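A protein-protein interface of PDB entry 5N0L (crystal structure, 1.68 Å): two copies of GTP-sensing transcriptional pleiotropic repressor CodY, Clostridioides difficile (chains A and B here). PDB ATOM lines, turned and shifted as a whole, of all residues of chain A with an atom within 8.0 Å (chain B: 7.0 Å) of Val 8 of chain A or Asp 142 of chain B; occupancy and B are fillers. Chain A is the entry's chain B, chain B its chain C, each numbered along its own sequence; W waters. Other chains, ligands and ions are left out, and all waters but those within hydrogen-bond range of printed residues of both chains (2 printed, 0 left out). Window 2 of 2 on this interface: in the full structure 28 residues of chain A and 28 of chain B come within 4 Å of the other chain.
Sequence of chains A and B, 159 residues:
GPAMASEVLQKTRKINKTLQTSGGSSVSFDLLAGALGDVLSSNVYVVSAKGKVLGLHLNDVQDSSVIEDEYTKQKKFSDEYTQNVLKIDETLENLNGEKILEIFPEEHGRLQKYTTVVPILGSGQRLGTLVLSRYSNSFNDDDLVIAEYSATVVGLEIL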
ATOM      1  N   ALA A   5      11.473 -18.787 -38.519  1.00  0.00           N
ATOM      2  CA  ALA A   5      11.255 -19.634 -37.379  1.00  0.00           C
ATOM      3  C   ALA A   5      11.891 -19.017 -36.167  1.00  0.00           C
ATOM      4  O   ALA A   5      12.916 -18.325 -36.261  1.00  0.00           O
ATOM      5  CB  ALA A   5      11.799 -21.004 -37.637  1.00  0.00           C
ATOM      6  N   SER A   6      11.286 -19.268 -35.015  1.00  0.00           N
ATOM      7  CA  SER A   6      11.828 -18.783 -33.784  1.00  0.00           C
ATOM      8  C   SER A   6      13.202 -19.423 -33.521  1.00  0.00           C
ATOM      9  O   SER A   6      13.546 -20.498 -34.023  1.00  0.00           O
ATOM     10  CB  SER A   6      10.918 -19.146 -32.619  1.00  0.00           C
ATOM     11  OG  SER A   6      10.967 -20.557 -32.467  1.00  0.00           O
ATOM     12  N   GLU A   7      13.969 -18.767 -32.682  1.00  0.00           N
ATOM     13  CA  GLU A   7      15.357 -19.278 -32.352  1.00  0.00           C
ATOM     14  C   GLU A   7      15.290 -20.745 -31.839  1.00  0.00           C
ATOM     15  O   GLU A   7      16.037 -21.623 -32.292  1.00  0.00           O
ATOM     16  CB  GLU A   7      15.998 -18.385 -31.310  1.00  0.00           C
ATOM     17  CG  GLU A   7      17.472 -18.731 -31.078  1.00  0.00           C
ATOM     18  CD  GLU A   7      18.328 -17.571 -30.610  1.00  0.00           C
ATOM     19  OE1 GLU A   7      18.337 -17.343 -29.373  1.00  0.00           O
ATOM     20  OE2 GLU A   7      19.012 -16.930 -31.466  1.00  0.00           O
ATOM     21  N   VAL A   8      14.361 -21.006 -30.906  1.00  0.00           N
ATOM     22  CA  VAL A   8      14.257 -22.333 -30.303  1.00  0.00           C
ATOM     23  C   VAL A   8      13.955 -23.349 -31.365  1.00  0.00           C
ATOM     24  O   VAL A   8      14.522 -24.441 -31.335  1.00  0.00           O
ATOM     25  CB  VAL A   8      13.254 -22.411 -29.114  1.00  0.00           C
ATOM     26  CG1 VAL A   8      11.769 -22.257 -29.555  1.00  0.00           C
ATOM     27  CG2 VAL A   8      13.375 -23.716 -28.366  1.00  0.00           C
ATOM     28  N   LEU A   9      13.071 -23.016 -32.291  1.00  0.00           N
ATOM     29  CA  LEU A   9      12.782 -23.937 -33.392  1.00  0.00           C
ATOM     30  C   LEU A   9      13.994 -24.116 -34.342  1.00  0.00           C
ATOM     31  O   LEU A   9      14.298 -25.193 -34.778  1.00  0.00           O
ATOM     32  CB  LEU A   9      11.553 -23.471 -34.176  1.00  0.00           C
ATOM     33  CG  LEU A   9      11.074 -24.321 -35.351  1.00  0.00           C
ATOM     34  CD1 LEU A   9      10.847 -25.749 -34.867  1.00  0.00           C
ATOM     35  CD2 LEU A   9       9.778 -23.702 -35.969  1.00  0.00           C
ATOM     36  N   GLN A  10      14.675 -23.048 -34.677  1.00  0.00           N
ATOM     37  CA  GLN A  10      15.892 -23.198 -35.525  1.00  0.00           C
ATOM     38  C   GLN A  10      16.950 -24.086 -34.837  1.00  0.00           C
ATOM     39  O   GLN A  10      17.616 -24.899 -35.484  1.00  0.00           O
ATOM     40  CB  GLN A  10      16.524 -21.819 -35.847  1.00  0.00           C
ATOM     41  CG  GLN A  10      15.729 -20.859 -36.718  1.00  0.00           C
ATOM     42  CD  GLN A  10      16.494 -19.556 -36.939  1.00  0.00           C
ATOM     43  OE1 GLN A  10      17.719 -19.565 -36.945  1.00  0.00           O
ATOM     44  NE2 GLN A  10      15.793 -18.451 -37.095  1.00  0.00           N
ATOM     45  N   LYS A  11      17.136 -23.904 -33.538  1.00  0.00           N
ATOM     46  CA  LYS A  11      18.157 -24.732 -32.804  1.00  0.00           C
ATOM     47  C   LYS A  11      17.710 -26.158 -32.700  1.00  0.00           C
ATOM     48  O   LYS A  11      18.466 -27.074 -32.892  1.00  0.00           O
ATOM     49  CB  LYS A  11      18.430 -24.170 -31.432  1.00  0.00           C
ATOM     50  CG  LYS A  11      19.136 -22.816 -31.474  1.00  0.00           C
ATOM     51  CD  LYS A  11      19.364 -22.191 -30.101  1.00  0.00           C
ATOM     52  CE  LYS A  11      20.310 -20.967 -30.245  1.00  0.00           C
ATOM     53  NZ  LYS A  11      20.632 -20.460 -28.896  1.00  0.00           N
ATOM     54  N   THR A  12      16.408 -26.348 -32.434  1.00  0.00           N
ATOM     55  CA  THR A  12      15.859 -27.702 -32.465  1.00  0.00           C
ATOM     56  C   THR A  12      16.093 -28.410 -33.816  1.00  0.00           C
ATOM     57  O   THR A  12      16.448 -29.600 -33.851  1.00  0.00           O
ATOM     58  CB  THR A  12      14.341 -27.630 -32.131  1.00  0.00           C
ATOM     59  OG1 THR A  12      14.243 -27.142 -30.814  1.00  0.00           O
ATOM     60  CG2 THR A  12      13.646 -29.047 -32.263  1.00  0.00           C
ATOM     61  N   ARG A  13      15.916 -27.667 -34.909  1.00  0.00           N
ATOM     62  CA  ARG A  13      16.076 -28.218 -36.222  1.00  0.00           C
ATOM     63  C   ARG A  13      17.518 -28.605 -36.506  1.00  0.00           C
ATOM     64  O   ARG A  13      17.735 -29.615 -37.195  1.00  0.00           O
ATOM     65  CB  ARG A  13      15.524 -27.287 -37.304  1.00  0.00           C
ATOM     66  CG  ARG A  13      13.965 -27.441 -37.472  1.00  0.00           C
ATOM     67  CD  ARG A  13      13.343 -26.265 -38.158  1.00  0.00           C
ATOM     68  NE  ARG A  13      11.954 -26.539 -38.394  1.00  0.00           N
ATOM     69  CZ  ARG A  13      11.015 -25.724 -38.905  1.00  0.00           C
ATOM     70  NH1 ARG A  13      11.261 -24.473 -39.304  1.00  0.00           N
ATOM     71  NH2 ARG A  13       9.758 -26.218 -39.010  1.00  0.00           N
ATOM     72  N   LYS A  14      18.467 -27.827 -35.961  1.00  0.00           N
ATOM     73  CA  LYS A  14      19.908 -28.173 -36.097  1.00  0.00           C
ATOM     74  C   LYS A  14      20.216 -29.443 -35.328  1.00  0.00           C
ATOM     75  O   LYS A  14      20.863 -30.353 -35.868  1.00  0.00           O
ATOM     76  CB  LYS A  14      20.841 -27.040 -35.600  1.00  0.00           C
ATOM     77  CG  LYS A  14      20.934 -25.855 -36.534  1.00  0.00           C
ATOM     78  CD  LYS A  14      22.103 -24.916 -36.206  1.00  0.00           C
ATOM     79  CE  LYS A  14      21.922 -23.562 -36.902  1.00  0.00           C
ATOM     80  NZ  LYS A  14      23.181 -22.757 -36.993  1.00  0.00           N
ATOM     81  N   ILE A  15      19.770 -29.514 -34.063  1.00  0.00           N
ATOM     82  CA  ILE A  15      19.947 -30.725 -33.268  1.00  0.00           C
ATOM     83  C   ILE A  15      19.310 -31.906 -34.008  1.00  0.00           C
ATOM     84  O   ILE A  15      19.919 -32.979 -34.147  1.00  0.00           O
ATOM     85  CB  ILE A  15      19.368 -30.624 -31.840  1.00  0.00           C
ATOM     86  CG1 ILE A  15      19.973 -29.487 -31.017  1.00  0.00           C
ATOM     87  CG2 ILE A  15      19.549 -31.910 -31.110  1.00  0.00           C
ATOM     88  CD1 ILE A  15      21.438 -29.689 -30.779  1.00  0.00           C
ATOM     89  N   LEU B  40      24.363 -23.990 -28.350  1.00  0.00           N
ATOM     90  CA  LEU B  40      24.408 -23.329 -27.042  1.00  0.00           C
ATOM     91  C   LEU B  40      25.703 -22.653 -26.730  1.00  0.00           C
ATOM     92  O   LEU B  40      25.846 -22.132 -25.631  1.00  0.00           O
ATOM     93  CB  LEU B  40      24.058 -24.311 -25.908  1.00  0.00           C
ATOM     94  CG  LEU B  40      22.692 -25.013 -26.165  1.00  0.00           C
ATOM     95  CD1 LEU B  40      22.444 -25.959 -25.015  1.00  0.00           C
ATOM     96  CD2 LEU B  40      21.586 -23.973 -26.258  1.00  0.00           C
ATOM     97  N   PHE B 139      21.616 -19.526 -19.176  1.00  0.00           N
ATOM     98  CA  PHE B 139      20.692 -20.349 -19.949  1.00  0.00           C
ATOM     99  C   PHE B 139      19.217 -19.945 -19.706  1.00  0.00           C
ATOM    100  O   PHE B 139      18.813 -19.706 -18.563  1.00  0.00           O
ATOM    101  CB  PHE B 139      20.925 -21.810 -19.570  1.00  0.00           C
ATOM    102  CG  PHE B 139      22.283 -22.349 -20.003  1.00  0.00           C
ATOM    103  CD1 PHE B 139      22.544 -22.688 -21.329  1.00  0.00           C
ATOM    104  CD2 PHE B 139      23.330 -22.469 -19.085  1.00  0.00           C
ATOM    105  CE1 PHE B 139      23.784 -23.197 -21.712  1.00  0.00           C
ATOM    106  CE2 PHE B 139      24.585 -22.982 -19.491  1.00  0.00           C
ATOM    107  CZ  PHE B 139      24.784 -23.339 -20.775  1.00  0.00           C
ATOM    108  N   ASN B 140      18.399 -19.936 -20.764  1.00  0.00           N
ATOM    109  CA  ASN B 140      16.986 -19.645 -20.616  1.00  0.00           C
ATOM    110  C   ASN B 140      16.212 -20.933 -20.864  1.00  0.00           C
ATOM    111  O   ASN B 140      16.763 -21.988 -21.086  1.00  0.00           O
ATOM    112  CB  ASN B 140      16.587 -18.455 -21.508  1.00  0.00           C
ATOM    113  CG  ASN B 140      16.640 -18.763 -22.976  1.00  0.00           C
ATOM    114  OD1 ASN B 140      16.720 -19.917 -23.413  1.00  0.00           O
ATOM    115  ND2 ASN B 140      16.612 -17.738 -23.748  1.00  0.00           N
ATOM    116  N   ASP B 141      14.896 -20.798 -20.850  1.00  0.00           N
ATOM    117  CA  ASP B 141      14.005 -21.982 -20.934  1.00  0.00           C
ATOM    118  C   ASP B 141      14.027 -22.637 -22.282  1.00  0.00           C
ATOM    119  O   ASP B 141      13.872 -23.845 -22.372  1.00  0.00           O
ATOM    120  CB  ASP B 141      12.574 -21.584 -20.543  1.00  0.00           C
ATOM    121  CG  ASP B 141      12.367 -21.436 -19.024  1.00  0.00           C
ATOM    122  OD1 ASP B 141      13.279 -21.652 -18.188  1.00  0.00           O
ATOM    123  OD2 ASP B 141      11.246 -21.055 -18.653  1.00  0.00           O
ATOM    124  N   ASP B 142      14.274 -21.846 -23.346  1.00  0.00           N
ATOM    125  CA  ASP B 142      14.465 -22.417 -24.676  1.00  0.00           C
ATOM    126  C   ASP B 142      15.737 -23.291 -24.699  1.00  0.00           C
ATOM    127  O   ASP B 142      15.755 -24.383 -25.280  1.00  0.00           O
ATOM    128  CB  ASP B 142      14.600 -21.336 -25.738  1.00  0.00           C
ATOM    129  CG  ASP B 142      13.285 -20.593 -26.051  1.00  0.00           C
ATOM    130  OD1 ASP B 142      12.111 -21.087 -25.780  1.00  0.00           O
ATOM    131  OD2 ASP B 142      13.479 -19.505 -26.633  1.00  0.00           O
ATOM    132  N   ASP B 143      16.787 -22.812 -24.043  1.00  0.00           N
ATOM    133  CA  ASP B 143      18.004 -23.604 -23.920  1.00  0.00           C
ATOM    134  C   ASP B 143      17.748 -24.878 -23.177  1.00  0.00           C
ATOM    135  O   ASP B 143      18.255 -25.934 -23.549  1.00  0.00           O
ATOM    136  CB  ASP B 143      19.139 -22.832 -23.219  1.00  0.00           C
ATOM    137  CG  ASP B 143      19.550 -21.577 -23.996  1.00  0.00           C
ATOM    138  OD1 ASP B 143      19.574 -21.567 -25.273  1.00  0.00           O
ATOM    139  OD2 ASP B 143      19.807 -20.577 -23.327  1.00  0.00           O
ATOM    140  N   LEU B 144      16.931 -24.785 -22.107  1.00  0.00           N
ATOM    141  CA  LEU B 144      16.537 -26.013 -21.357  1.00  0.00           C
ATOM    142  C   LEU B 144      15.744 -27.019 -22.176  1.00  0.00           C
ATOM    143  O   LEU B 144      15.935 -28.217 -22.016  1.00  0.00           O
ATOM    144  CB  LEU B 144      15.913 -25.693 -20.049  1.00  0.00           C
ATOM    145  CG  LEU B 144      16.724 -24.919 -19.012  1.00  0.00           C
ATOM    146  CD1 LEU B 144      15.896 -24.650 -17.776  1.00  0.00           C
ATOM    147  CD2 LEU B 144      17.993 -25.687 -18.653  1.00  0.00           C
ATOM    148  N   VAL B 145      14.889 -26.530 -23.084  1.00  0.00           N
ATOM    149  CA  VAL B 145      14.201 -27.426 -23.992  1.00  0.00           C
ATOM    150  C   VAL B 145      15.184 -28.266 -24.770  1.00  0.00           C
ATOM    151  O   VAL B 145      15.139 -29.460 -24.794  1.00  0.00           O
ATOM    152  CB  VAL B 145      13.288 -26.679 -24.937  1.00  0.00           C
ATOM    153  CG1 VAL B 145      12.631 -27.593 -25.974  1.00  0.00           C
ATOM    154  CG2 VAL B 145      12.175 -26.013 -24.133  1.00  0.00           C
ATOM    155  N   ILE B 146      16.184 -27.582 -25.343  1.00  0.00           N
ATOM    156  CA  ILE B 146      17.158 -28.242 -26.171  1.00  0.00           C
ATOM    157  C   ILE B 146      18.002 -29.214 -25.355  1.00  0.00           C
ATOM    158  O   ILE B 146      18.187 -30.359 -25.776  1.00  0.00           O
ATOM    159  CB  ILE B 146      18.004 -27.203 -26.943  1.00  0.00           C
ATOM    160  CG1 ILE B 146      17.107 -26.445 -27.947  1.00  0.00           C
ATOM    161  CG2 ILE B 146      19.151 -27.917 -27.676  1.00  0.00           C
ATOM    162  CD1 ILE B 146      17.713 -25.122 -28.273  1.00  0.00           C
ATOM    163  N   ALA B 147      18.446 -28.781 -24.170  1.00  0.00           N
ATOM    164  CA  ALA B 147      19.255 -29.613 -23.275  1.00  0.00           C
ATOM    165  C   ALA B 147      18.539 -30.848 -22.810  1.00  0.00           C
ATOM    166  O   ALA B 147      19.054 -31.924 -22.776  1.00  0.00           O
ATOM    167  CB  ALA B 147      19.759 -28.809 -22.092  1.00  0.00           C
ATOM    168  N   TYR B 149      15.686 -32.320 -24.058  1.00  0.00           N
ATOM    169  CA  TYR B 149      15.331 -33.310 -25.015  1.00  0.00           C
ATOM    170  C   TYR B 149      16.604 -34.038 -25.567  1.00  0.00           C
ATOM    171  O   TYR B 149      16.588 -35.221 -25.790  1.00  0.00           O
ATOM    172  CB  TYR B 149      14.331 -32.838 -26.053  1.00  0.00           C
ATOM    173  CG  TYR B 149      14.858 -32.387 -27.381  1.00  0.00           C
ATOM    174  CD1 TYR B 149      15.313 -33.293 -28.348  1.00  0.00           C
ATOM    175  CD2 TYR B 149      14.730 -31.055 -27.732  1.00  0.00           C
ATOM    176  CE1 TYR B 149      15.773 -32.840 -29.611  1.00  0.00           C
ATOM    177  CE2 TYR B 149      15.137 -30.599 -28.970  1.00  0.00           C
ATOM    178  CZ  TYR B 149      15.645 -31.494 -29.913  1.00  0.00           C
ATOM    179  OH  TYR B 149      16.043 -30.922 -31.145  1.00  0.00           O
HETATM  180  O   HOH W   1      17.774 -20.610 -27.332  1.00  0.00           O
HETATM  181  O   HOH W   2      12.839 -18.924 -29.332  1.00  0.00           O
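The side-chain amino group of Lys 11 of chain A lies within salt-bridge range of the side-chain carboxylate of Asp 143 of chain B (3.9 Å). O of Thr 12 of chain A lies within hydrogen-bond range of OH of Tyr 149 of chain B (3.0 Å).
The side-chain amino group (NZ) of Lys 11 of chain A is in salt-bridge range of the side-chain carboxylate (OE1) of Glu 7 of chain A. The backbone carbonyl oxygen (O) of Val 8 of chain A lies within hydrogen-bond range of the side-chain hydroxyl (OG1) of Thr 12 of chain A, at 2.8 Å. OD1 of Asn 140 of chain B sits at hydrogen-bond distance from N of Asp 142 of chain B. OD1 of Asn 140 of chain B is in hydrogen-bond range of N of Asp 143 of chain B (3.0 Å).
Among the printed residues, pairs that only touch across the chains: Val 8 of chain A with Asp 142 of chain B, Lys 11 of chain A with Ile 146 of chain B, Ile 15 of chain A with Ile 146 of chain B and Ile 15 of chain A with Tyr 149 of chain B.
Of chain B, only Asp 142 comes within 4 Å of Val 8 of chain A. Of the printed residues of chain B, Lys 11 of chain A touches Asp 143 and Ile 146. Asp 142 of chain B touches just one residue of chain A: Val 8. Of the printed residues of chain A, Asp 143 of chain B touches Lys 11. Of the printed residues of chain A, Ile 146 of chain B touches Lys 11 (3.4 Å) and Ile 15 (3.8 Å). The nearest residue of chain B that does not touch Val 8 of chain A is Ile 146 of chain B (4.5 Å). The nearest printed residue of chain B that does not touch Thr 12 of chain A is Ile 146 of chain B (4.1 Å).
Hydrophobic or aromatic side chains of chain A within 4 Å of the printed part of chain B: Val 8 and Ile 15. Among the printed residues, Asp or Glu carboxylates within 4 Å of a Lys or Arg side-chain nitrogen of the other chain: Lys 11 of chain A with Asp 143 of chain B (3.9 Å).
No position is printed for both chains. Of the 6 pairs that touch across the chains among the printed residues, none has its exchanged pair printed and touching as well.
Water W2 bridges the side-chain carboxylate (OD2) of Asp 142 of chain B (2.8 Å) and the backbone NH (N) of Val 8 of chain A (3.0 Å). Water W1 lies within hydrogen-bond range of OD1 of Asp 143 of chain B (2.9 Å) and NZ of Lys 11 of chain A (3.3 Å).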
